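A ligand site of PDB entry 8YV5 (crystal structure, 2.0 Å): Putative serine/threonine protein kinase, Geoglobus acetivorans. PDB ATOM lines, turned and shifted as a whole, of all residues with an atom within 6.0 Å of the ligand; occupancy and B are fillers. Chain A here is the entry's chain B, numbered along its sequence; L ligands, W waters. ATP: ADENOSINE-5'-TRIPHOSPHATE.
Val 8 touches the ligand.
Ala 15 touches the ligand.
CG of Pro 44 touches N6 of the ligand, at 3.8 Å.
CA of Phe 60 touches N1 of the ligand, at 3.6 Å.
Ile 114 touches the ligand (CD1 to C8, 3.7 Å).
Hydrophobic or aromatic side chains that line the ligand: Val 8, Ala 15, Pro 44, Met 58, Phe 60, Ile 61, His 104 and Ile 114.
Water W5 bridges an oxygen (O1B) of the ligand (2.7 Å) and the backbone carbonyl oxygen (O) of Ser 6 (2.9 Å).
Water W2 bridges an oxygen (O2') of the ligand (2.7 Å) and the backbone carbonyl oxygen (O) of Arg 103 (2.8 Å).
Water W4 bridges an oxygen (O2G) of the ligand and the guanidinium group (NH1) of Arg 118.
NZ of Lys 17 is in salt-bridge range of O2A of the ligand (2.9 Å).
An oxygen (O2B) of the ligand lies within hydrogen-bond range of the side-chain hydroxyl (OG) of Ser 6, at 2.7 Å.
The guanidinium group of Arg 118 is in salt-bridge range of an oxygen (O1G) of the ligand (2.7 Å).
The backbone NH (N) of His 5 sits at hydrogen-bond distance from an oxygen (O3G) of the ligand (3.2 Å).
The side-chain carboxylate (OE1) of Glu 117 lies close to an oxygen (O1G) of the ligand, 3.0 Å away.
The guanidinium group (NH1) of Arg 103 is in salt-bridge range of an oxygen (O1A) of the ligand.
An oxygen (O1A) of the ligand is in hydrogen-bond range of a ring nitrogen (NE2) of His 104.
An oxygen (O1B) of the ligand lies within salt-bridge range of the guanidinium group of Arg 4 (2.8 Å).
An oxygen (O1G) of the ligand sits close to the side-chain carboxylate of Asp 115 (2.7 Å).
N6 of the ligand lies within hydrogen-bond range of O of Glu 59 (2.9 Å).
N of Ser 6 lies within hydrogen-bond range of O2B of the ligand.
A nitrogen (N1) of the ligand lies within hydrogen-bond range of the backbone NH (N) of Ile 61, at 2.8 Å.
A nitrogen (N6) of the ligand lies within hydrogen-bond range of the side-chain sulfur (SD) of Met 58, 3.5 Å away.
NH1 of Arg 118 lies within salt-bridge range of OE2 of Glu 117, 3.3 Å away.
The side-chain carboxylate (OD1) of Asp 115 is in salt-bridge range of the side-chain amino group (NZ) of Lys 17 (3.0 Å).
NH2 of Arg 118 is in hydrogen-bond range of ND1 of His 5.
The backbone carbonyl oxygen (O) of His 104 lies within hydrogen-bond range of the backbone NH (N) of Ile 114, 2.9 Å away.
The side-chain amino group (NZ) of Lys 17 is in salt-bridge range of the side-chain carboxylate (OE1) of Glu 30, 2.7 Å away.
A ring nitrogen (NE2) of His 104 sits at hydrogen-bond distance from the guanidinium group of Arg 103, 3.5 Å away.
The backbone carbonyl oxygen of Met 58 is in hydrogen-bond range of the backbone NH of Ala 15 (2.8 Å).
The side-chain amino group (NZ) of Lys 17 is in salt-bridge range of the side-chain carboxylate (OE1) of Glu 117 (3.1 Å).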
ATOM      1  N   GLY A   3      -9.192 -10.535  -5.903  1.00  0.00           N
ATOM      2  CA  GLY A   3      -9.797 -11.683  -6.548  1.00  0.00           C
ATOM      3  C   GLY A   3     -10.133 -11.445  -8.013  1.00  0.00           C
ATOM      4  O   GLY A   3     -11.229 -10.976  -8.345  1.00  0.00           O
ATOM      5  N   ARG A   4      -9.185 -11.743  -8.895  1.00  0.00           N
ATOM      6  CA  ARG A   4      -9.331 -11.491 -10.323  1.00  0.00           C
ATOM      7  C   ARG A   4      -9.755 -12.775 -11.045  1.00  0.00           C
ATOM      8  O   ARG A   4      -9.541 -13.886 -10.566  1.00  0.00           O
ATOM      9  CB  ARG A   4      -8.034 -10.941 -10.933  1.00  0.00           C
ATOM     10  CG  ARG A   4      -7.523  -9.622 -10.324  1.00  0.00           C
ATOM     11  CD  ARG A   4      -8.297  -8.397 -10.791  1.00  0.00           C
ATOM     12  NE  ARG A   4      -7.715  -7.184 -10.225  1.00  0.00           N
ATOM     13  CZ  ARG A   4      -6.772  -6.447 -10.814  1.00  0.00           C
ATOM     14  NH1 ARG A   4      -6.338  -6.725 -12.036  1.00  0.00           N
ATOM     15  NH2 ARG A   4      -6.235  -5.423 -10.142  1.00  0.00           N
ATOM     16  N   HIS A   5     -10.367 -12.603 -12.216  1.00  0.00           N
ATOM     17  CA  HIS A   5     -10.843 -13.737 -12.987  1.00  0.00           C
ATOM     18  C   HIS A   5      -9.866 -14.180 -14.065  1.00  0.00           C
ATOM     19  O   HIS A   5     -10.105 -15.193 -14.730  1.00  0.00           O
ATOM     20  CB  HIS A   5     -12.183 -13.388 -13.644  1.00  0.00           C
ATOM     21  CG  HIS A   5     -13.353 -13.460 -12.713  1.00  0.00           C
ATOM     22  ND1 HIS A   5     -14.524 -12.758 -12.919  1.00  0.00           N
ATOM     23  CD2 HIS A   5     -13.529 -14.116 -11.546  1.00  0.00           C
ATOM     24  CE1 HIS A   5     -15.381 -13.015 -11.948  1.00  0.00           C
ATOM     25  NE2 HIS A   5     -14.797 -13.829 -11.091  1.00  0.00           N
ATOM     26  N   SER A   6      -8.750 -13.471 -14.226  1.00  0.00           N
ATOM     27  CA  SER A   6      -7.908 -13.677 -15.392  1.00  0.00           C
ATOM     28  C   SER A   6      -6.506 -13.164 -15.091  1.00  0.00           C
ATOM     29  O   SER A   6      -6.284 -12.470 -14.101  1.00  0.00           O
ATOM     30  CB  SER A   6      -8.509 -12.950 -16.599  1.00  0.00           C
ATOM     31  OG  SER A   6      -8.310 -11.545 -16.461  1.00  0.00           O
ATOM     32  N   VAL A   7      -5.571 -13.544 -15.942  1.00  0.00           N
ATOM     33  CA  VAL A   7      -4.252 -12.918 -16.013  1.00  0.00           C
ATOM     34  C   VAL A   7      -4.152 -12.281 -17.403  1.00  0.00           C
ATOM     35  O   VAL A   7      -4.484 -12.936 -18.400  1.00  0.00           O
ATOM     36  CB  VAL A   7      -3.126 -13.949 -15.824  1.00  0.00           C
ATOM     37  CG1 VAL A   7      -1.767 -13.286 -16.043  1.00  0.00           C
ATOM     38  CG2 VAL A   7      -3.255 -14.602 -14.504  1.00  0.00           C
ATOM     39  N   VAL A   8      -3.718 -11.020 -17.451  1.00  0.00           N
ATOM     40  CA  VAL A   8      -3.535 -10.320 -18.721  1.00  0.00           C
ATOM     41  C   VAL A   8      -2.048 -10.171 -18.954  1.00  0.00           C
ATOM     42  O   VAL A   8      -1.306  -9.713 -18.072  1.00  0.00           O
ATOM     43  CB  VAL A   8      -4.262  -8.970 -18.756  1.00  0.00           C
ATOM     44  CG1 VAL A   8      -3.886  -8.196 -20.029  1.00  0.00           C
ATOM     45  CG2 VAL A   8      -5.814  -9.199 -18.730  1.00  0.00           C
ATOM     46  N   ALA A  15      -3.112  -7.289 -26.096  1.00  0.00           N
ATOM     47  CA  ALA A  15      -3.371  -7.719 -24.737  1.00  0.00           C
ATOM     48  C   ALA A  15      -3.979  -9.105 -24.846  1.00  0.00           C
ATOM     49  O   ALA A  15      -4.924  -9.325 -25.619  1.00  0.00           O
ATOM     50  CB  ALA A  15      -4.345  -6.754 -24.059  1.00  0.00           C
ATOM     51  N   LYS A  17      -5.792 -11.877 -22.629  1.00  0.00           N
ATOM     52  CA  LYS A  17      -6.459 -12.090 -21.350  1.00  0.00           C
ATOM     53  C   LYS A  17      -6.774 -13.572 -21.222  1.00  0.00           C
ATOM     54  O   LYS A  17      -7.533 -14.112 -22.036  1.00  0.00           O
ATOM     55  CB  LYS A  17      -7.731 -11.259 -21.262  1.00  0.00           C
ATOM     56  CG  LYS A  17      -8.467 -11.384 -19.952  1.00  0.00           C
ATOM     57  CD  LYS A  17      -9.618 -10.343 -19.929  1.00  0.00           C
ATOM     58  CE  LYS A  17     -10.283 -10.237 -18.539  1.00  0.00           C
ATOM     59  NZ  LYS A  17     -11.288  -9.084 -18.517  1.00  0.00           N
ATOM     60  N   PHE A  19      -8.395 -16.410 -18.903  1.00  0.00           N
ATOM     61  CA  PHE A  19      -9.276 -16.641 -17.753  1.00  0.00           C
ATOM     62  C   PHE A  19      -8.887 -17.896 -16.985  1.00  0.00           C
ATOM     63  O   PHE A  19      -8.483 -18.912 -17.562  1.00  0.00           O
ATOM     64  CB  PHE A  19     -10.728 -16.746 -18.216  1.00  0.00           C
ATOM     65  CG  PHE A  19     -11.318 -15.423 -18.666  1.00  0.00           C
ATOM     66  CD1 PHE A  19     -11.042 -14.905 -19.917  1.00  0.00           C
ATOM     67  CD2 PHE A  19     -12.121 -14.707 -17.822  1.00  0.00           C
ATOM     68  CE1 PHE A  19     -11.575 -13.661 -20.341  1.00  0.00           C
ATOM     69  CE2 PHE A  19     -12.644 -13.484 -18.209  1.00  0.00           C
ATOM     70  CZ  PHE A  19     -12.383 -12.957 -19.476  1.00  0.00           C
ATOM     71  N   GLU A  30     -17.027 -11.994 -22.033  1.00  0.00           N
ATOM     72  CA  GLU A  30     -16.034 -11.076 -22.591  1.00  0.00           C
ATOM     73  C   GLU A  30     -15.969 -11.172 -24.113  1.00  0.00           C
ATOM     74  O   GLU A  30     -16.094 -10.162 -24.821  1.00  0.00           O
ATOM     75  CB  GLU A  30     -14.658 -11.363 -21.966  1.00  0.00           C
ATOM     76  CG  GLU A  30     -13.561 -10.372 -22.400  1.00  0.00           C
ATOM     77  CD  GLU A  30     -13.565  -9.135 -21.518  1.00  0.00           C
ATOM     78  OE1 GLU A  30     -13.349  -9.264 -20.287  1.00  0.00           O
ATOM     79  OE2 GLU A  30     -13.839  -8.032 -22.059  1.00  0.00           O
ATOM     80  N   PRO A  44     -11.700  -2.347 -27.409  1.00  0.00           N
ATOM     81  CA  PRO A  44     -10.551  -2.881 -28.172  1.00  0.00           C
ATOM     82  C   PRO A  44     -10.985  -3.708 -29.371  1.00  0.00           C
ATOM     83  O   PRO A  44     -12.032  -4.351 -29.345  1.00  0.00           O
ATOM     84  CB  PRO A  44      -9.815  -3.770 -27.156  1.00  0.00           C
ATOM     85  CG  PRO A  44     -10.354  -3.327 -25.809  1.00  0.00           C
ATOM     86  CD  PRO A  44     -11.755  -2.881 -26.031  1.00  0.00           C
ATOM     87  N   MET A  58      -6.633  -9.289 -28.007  1.00  0.00           N
ATOM     88  CA  MET A  58      -7.293  -8.069 -28.418  1.00  0.00           C
ATOM     89  C   MET A  58      -6.269  -6.943 -28.502  1.00  0.00           C
ATOM     90  O   MET A  58      -5.121  -7.071 -28.101  1.00  0.00           O
ATOM     91  CB  MET A  58      -8.364  -7.535 -27.443  1.00  0.00           C
ATOM     92  CG  MET A  58      -7.888  -7.398 -26.024  1.00  0.00           C
ATOM     93  SD  MET A  58      -9.184  -6.876 -24.881  1.00  0.00           S
ATOM     94  CE  MET A  58      -8.971  -8.228 -23.683  1.00  0.00           C
ATOM     95  N   GLU A  59      -6.729  -5.815 -29.023  1.00  0.00           N
ATOM     96  CA  GLU A  59      -5.889  -4.635 -29.118  1.00  0.00           C
ATOM     97  C   GLU A  59      -5.474  -4.148 -27.738  1.00  0.00           C
ATOM     98  O   GLU A  59      -6.311  -3.962 -26.847  1.00  0.00           O
ATOM     99  CB  GLU A  59      -6.687  -3.552 -29.850  1.00  0.00           C
ATOM    100  CG  GLU A  59      -6.012  -2.201 -30.084  1.00  0.00           C
ATOM    101  CD  GLU A  59      -7.035  -1.149 -30.489  1.00  0.00           C
ATOM    102  OE1 GLU A  59      -8.272  -1.403 -30.445  1.00  0.00           O
ATOM    103  OE2 GLU A  59      -6.610  -0.047 -30.851  1.00  0.00           O
ATOM    104  N   PHE A  60      -4.166  -3.897 -27.555  1.00  0.00           N
ATOM    105  CA  PHE A  60      -3.711  -3.159 -26.370  1.00  0.00           C
ATOM    106  C   PHE A  60      -4.048  -1.668 -26.516  1.00  0.00           C
ATOM    107  O   PHE A  60      -3.633  -1.004 -27.489  1.00  0.00           O
ATOM    108  CB  PHE A  60      -2.198  -3.330 -26.148  1.00  0.00           C
ATOM    109  CG  PHE A  60      -1.713  -2.769 -24.833  1.00  0.00           C
ATOM    110  CD1 PHE A  60      -1.487  -1.399 -24.686  1.00  0.00           C
ATOM    111  CD2 PHE A  60      -1.548  -3.583 -23.730  1.00  0.00           C
ATOM    112  CE1 PHE A  60      -1.045  -0.880 -23.473  1.00  0.00           C
ATOM    113  CE2 PHE A  60      -1.117  -3.046 -22.504  1.00  0.00           C
ATOM    114  CZ  PHE A  60      -0.887  -1.675 -22.394  1.00  0.00           C
ATOM    115  N   ILE A  61      -4.744  -1.145 -25.525  1.00  0.00           N
ATOM    116  CA  ILE A  61      -5.138   0.268 -25.542  1.00  0.00           C
ATOM    117  C   ILE A  61      -4.088   1.063 -24.777  1.00  0.00           C
ATOM    118  O   ILE A  61      -3.919   0.882 -23.569  1.00  0.00           O
ATOM    119  CB  ILE A  61      -6.519   0.472 -24.927  1.00  0.00           C
ATOM    120  CG1 ILE A  61      -7.533  -0.547 -25.507  1.00  0.00           C
ATOM    121  CG2 ILE A  61      -6.992   1.939 -25.167  1.00  0.00           C
ATOM    122  CD1 ILE A  61      -7.714  -0.466 -27.106  1.00  0.00           C
ATOM    123  N   GLU A  62      -3.416   1.974 -25.476  1.00  0.00           N
ATOM    124  CA  GLU A  62      -2.474   2.903 -24.854  1.00  0.00           C
ATOM    125  C   GLU A  62      -3.265   4.060 -24.259  1.00  0.00           C
ATOM    126  O   GLU A  62      -4.084   4.671 -24.937  1.00  0.00           O
ATOM    127  CB  GLU A  62      -1.544   3.419 -25.946  1.00  0.00           C
ATOM    128  CG  GLU A  62      -0.642   2.312 -26.510  1.00  0.00           C
ATOM    129  CD  GLU A  62       0.030   2.758 -27.790  1.00  0.00           C
ATOM    130  OE1 GLU A  62      -0.688   2.940 -28.790  1.00  0.00           O
ATOM    131  OE2 GLU A  62       1.232   2.987 -27.765  1.00  0.00           O
ATOM    132  N   ARG A 103      -9.952   1.099 -13.382  1.00  0.00           N
ATOM    133  CA  ARG A 103      -8.976   0.448 -14.235  1.00  0.00           C
ATOM    134  C   ARG A 103      -9.493   0.201 -15.637  1.00  0.00           C
ATOM    135  O   ARG A 103      -8.720  -0.262 -16.493  1.00  0.00           O
ATOM    136  CB  ARG A 103      -8.586  -0.925 -13.629  1.00  0.00           C
ATOM    137  CG  ARG A 103      -8.002  -0.833 -12.211  1.00  0.00           C
ATOM    138  CD  ARG A 103      -7.660  -2.234 -11.667  1.00  0.00           C
ATOM    139  NE  ARG A 103      -8.816  -3.088 -11.394  1.00  0.00           N
ATOM    140  CZ  ARG A 103      -9.129  -4.162 -12.121  1.00  0.00           C
ATOM    141  NH1 ARG A 103      -8.420  -4.503 -13.176  1.00  0.00           N
ATOM    142  NH2 ARG A 103     -10.174  -4.911 -11.770  1.00  0.00           N
ATOM    143  N   HIS A 104     -10.762   0.521 -15.917  1.00  0.00           N
ATOM    144  CA  HIS A 104     -11.472  -0.003 -17.083  1.00  0.00           C
ATOM    145  C   HIS A 104     -11.913   1.048 -18.085  1.00  0.00           C
ATOM    146  O   HIS A 104     -12.563   0.721 -19.086  1.00  0.00           O
ATOM    147  CB  HIS A 104     -12.663  -0.813 -16.559  1.00  0.00           C
ATOM    148  CG  HIS A 104     -12.230  -2.049 -15.818  1.00  0.00           C
ATOM    149  ND1 HIS A 104     -13.027  -2.694 -14.903  1.00  0.00           N
ATOM    150  CD2 HIS A 104     -11.129  -2.824 -15.957  1.00  0.00           C
ATOM    151  CE1 HIS A 104     -12.401  -3.757 -14.427  1.00  0.00           C
ATOM    152  NE2 HIS A 104     -11.253  -3.885 -15.076  1.00  0.00           N
ATOM    153  N   ILE A 106      -9.851   3.794 -20.314  1.00  0.00           N
ATOM    154  CA  ILE A 106      -8.466   4.103 -20.635  1.00  0.00           C
ATOM    155  C   ILE A 106      -8.486   5.322 -21.552  1.00  0.00           C
ATOM    156  O   ILE A 106      -9.168   5.311 -22.581  1.00  0.00           O
ATOM    157  CB  ILE A 106      -7.767   2.888 -21.281  1.00  0.00           C
ATOM    158  CG1 ILE A 106      -7.872   1.690 -20.298  1.00  0.00           C
ATOM    159  CG2 ILE A 106      -6.274   3.217 -21.672  1.00  0.00           C
ATOM    160  CD1 ILE A 106      -6.991   0.504 -20.638  1.00  0.00           C
ATOM    161  N   ILE A 114     -12.748  -1.189 -21.276  1.00  0.00           N
ATOM    162  CA  ILE A 114     -12.257  -2.593 -21.284  1.00  0.00           C
ATOM    163  C   ILE A 114     -12.954  -3.400 -20.171  1.00  0.00           C
ATOM    164  O   ILE A 114     -13.529  -2.776 -19.280  1.00  0.00           O
ATOM    165  CB  ILE A 114     -10.722  -2.640 -21.123  1.00  0.00           C
ATOM    166  CG1 ILE A 114     -10.273  -2.076 -19.772  1.00  0.00           C
ATOM    167  CG2 ILE A 114     -10.026  -1.948 -22.280  1.00  0.00           C
ATOM    168  CD1 ILE A 114      -8.909  -2.565 -19.337  1.00  0.00           C
ATOM    169  N   ASP A 115     -12.909  -4.730 -20.257  1.00  0.00           N
ATOM    170  CA  ASP A 115     -13.447  -5.623 -19.193  1.00  0.00           C
ATOM    171  C   ASP A 115     -14.969  -5.762 -19.266  1.00  0.00           C
ATOM    172  O   ASP A 115     -15.664  -5.104 -18.499  1.00  0.00           O
ATOM    173  CB  ASP A 115     -12.958  -5.262 -17.793  1.00  0.00           C
ATOM    174  CG  ASP A 115     -12.959  -6.471 -16.869  1.00  0.00           C
ATOM    175  OD1 ASP A 115     -13.529  -7.494 -17.263  1.00  0.00           O
ATOM    176  OD2 ASP A 115     -12.383  -6.367 -15.786  1.00  0.00           O
ATOM    177  N   GLU A 117     -16.388  -8.890 -19.085  1.00  0.00           N
ATOM    178  CA  GLU A 117     -16.653 -10.288 -18.716  1.00  0.00           C
ATOM    179  C   GLU A 117     -17.819 -10.405 -17.743  1.00  0.00           C
ATOM    180  O   GLU A 117     -18.288 -11.517 -17.527  1.00  0.00           O
ATOM    181  CB  GLU A 117     -15.436 -10.900 -18.054  1.00  0.00           C
ATOM    182  CG  GLU A 117     -15.164 -10.225 -16.741  1.00  0.00           C
ATOM    183  CD  GLU A 117     -14.069 -10.860 -15.971  1.00  0.00           C
ATOM    184  OE1 GLU A 117     -12.892 -10.734 -16.467  1.00  0.00           O
ATOM    185  OE2 GLU A 117     -14.357 -11.386 -14.859  1.00  0.00           O
ATOM    186  N   ARG A 118     -18.278  -9.322 -17.134  1.00  0.00           N
ATOM    187  CA  ARG A 118     -19.445  -9.447 -16.228  1.00  0.00           C
ATOM    188  C   ARG A 118     -20.705  -8.847 -16.854  1.00  0.00           C
ATOM    189  O   ARG A 118     -21.690  -8.687 -16.129  1.00  0.00           O
ATOM    190  CB  ARG A 118     -19.158  -8.776 -14.889  1.00  0.00           C
ATOM    191  CG  ARG A 118     -18.238  -9.571 -13.974  1.00  0.00           C
ATOM    192  CD  ARG A 118     -17.837  -8.727 -12.772  1.00  0.00           C
ATOM    193  NE  ARG A 118     -16.685  -9.268 -12.069  1.00  0.00           N
ATOM    194  CZ  ARG A 118     -15.422  -9.106 -12.451  1.00  0.00           C
ATOM    195  NH1 ARG A 118     -15.145  -8.430 -13.555  1.00  0.00           N
ATOM    196  NH2 ARG A 118     -14.446  -9.620 -11.729  1.00  0.00           N
HETATM  197  PG  ATP L   1     -11.694  -8.339 -13.240  1.00  0.00           P
HETATM  198  O1G ATP L   1     -12.578  -8.653 -14.389  1.00  0.00           O
HETATM  199  O2G ATP L   1     -12.210  -7.183 -12.422  1.00  0.00           O
HETATM  200  O3G ATP L   1     -11.383  -9.550 -12.411  1.00  0.00           O
HETATM  201  PB  ATP L   1      -9.111  -8.640 -14.518  1.00  0.00           P
HETATM  202  O1B ATP L   1      -7.853  -8.168 -13.901  1.00  0.00           O
HETATM  203  O2B ATP L   1      -9.453 -10.086 -14.510  1.00  0.00           O
HETATM  204  O3B ATP L   1     -10.312  -7.821 -13.859  1.00  0.00           O
HETATM  205  PA  ATP L   1      -8.997  -6.699 -16.727  1.00  0.00           P
HETATM  206  O1A ATP L   1      -9.250  -5.633 -15.724  1.00  0.00           O
HETATM  207  O2A ATP L   1      -9.794  -6.690 -17.979  1.00  0.00           O
HETATM  208  O3A ATP L   1      -9.190  -8.121 -16.033  1.00  0.00           O
HETATM  209  O5' ATP L   1      -7.442  -6.739 -17.091  1.00  0.00           O
HETATM  210  C5' ATP L   1      -6.461  -6.486 -16.077  1.00  0.00           C
HETATM  211  C4' ATP L   1      -5.665  -5.261 -16.441  1.00  0.00           C
HETATM  212  O4' ATP L   1      -4.992  -5.480 -17.707  1.00  0.00           O
HETATM  213  C3' ATP L   1      -6.474  -3.977 -16.655  1.00  0.00           C
HETATM  214  O3' ATP L   1      -6.737  -3.326 -15.420  1.00  0.00           O
HETATM  215  C2' ATP L   1      -5.522  -3.175 -17.542  1.00  0.00           C
HETATM  216  O2' ATP L   1      -4.499  -2.561 -16.798  1.00  0.00           O
HETATM  217  C1' ATP L   1      -4.947  -4.270 -18.441  1.00  0.00           C
HETATM  218  N9  ATP L   1      -5.670  -4.473 -19.689  1.00  0.00           N
HETATM  219  C8  ATP L   1      -6.634  -5.399 -19.961  1.00  0.00           C
HETATM  220  N7  ATP L   1      -7.077  -5.332 -21.194  1.00  0.00           N
HETATM  221  C5  ATP L   1      -6.329  -4.308 -21.770  1.00  0.00           C
HETATM  222  C6  ATP L   1      -6.323  -3.754 -23.061  1.00  0.00           C
HETATM  223  N6  ATP L   1      -7.113  -4.164 -24.056  1.00  0.00           N
HETATM  224  N1  ATP L   1      -5.463  -2.732 -23.293  1.00  0.00           N
HETATM  225  C2  ATP L   1      -4.673  -2.322 -22.298  1.00  0.00           C
HETATM  226  N3  ATP L   1      -4.589  -2.769 -21.049  1.00  0.00           N
HETATM  227  C4  ATP L   1      -5.457  -3.778 -20.849  1.00  0.00           C
HETATM  228  O   HOH W   1      -4.348  -2.938 -13.355  1.00  0.00           O
HETATM  229  O   HOH W   2      -5.913  -0.265 -16.358  1.00  0.00           O
HETATM  230  O   HOH W   3      -9.614  -6.525 -20.834  1.00  0.00           O
HETATM  231  O   HOH W   4     -14.419  -5.473 -12.459  1.00  0.00           O
HETATM  232  O   HOH W   5      -5.641  -9.676 -14.025  1.00  0.00           O
HETATM  233  O   HOH W   6      -2.961  -1.229 -19.269  1.00  0.00           O
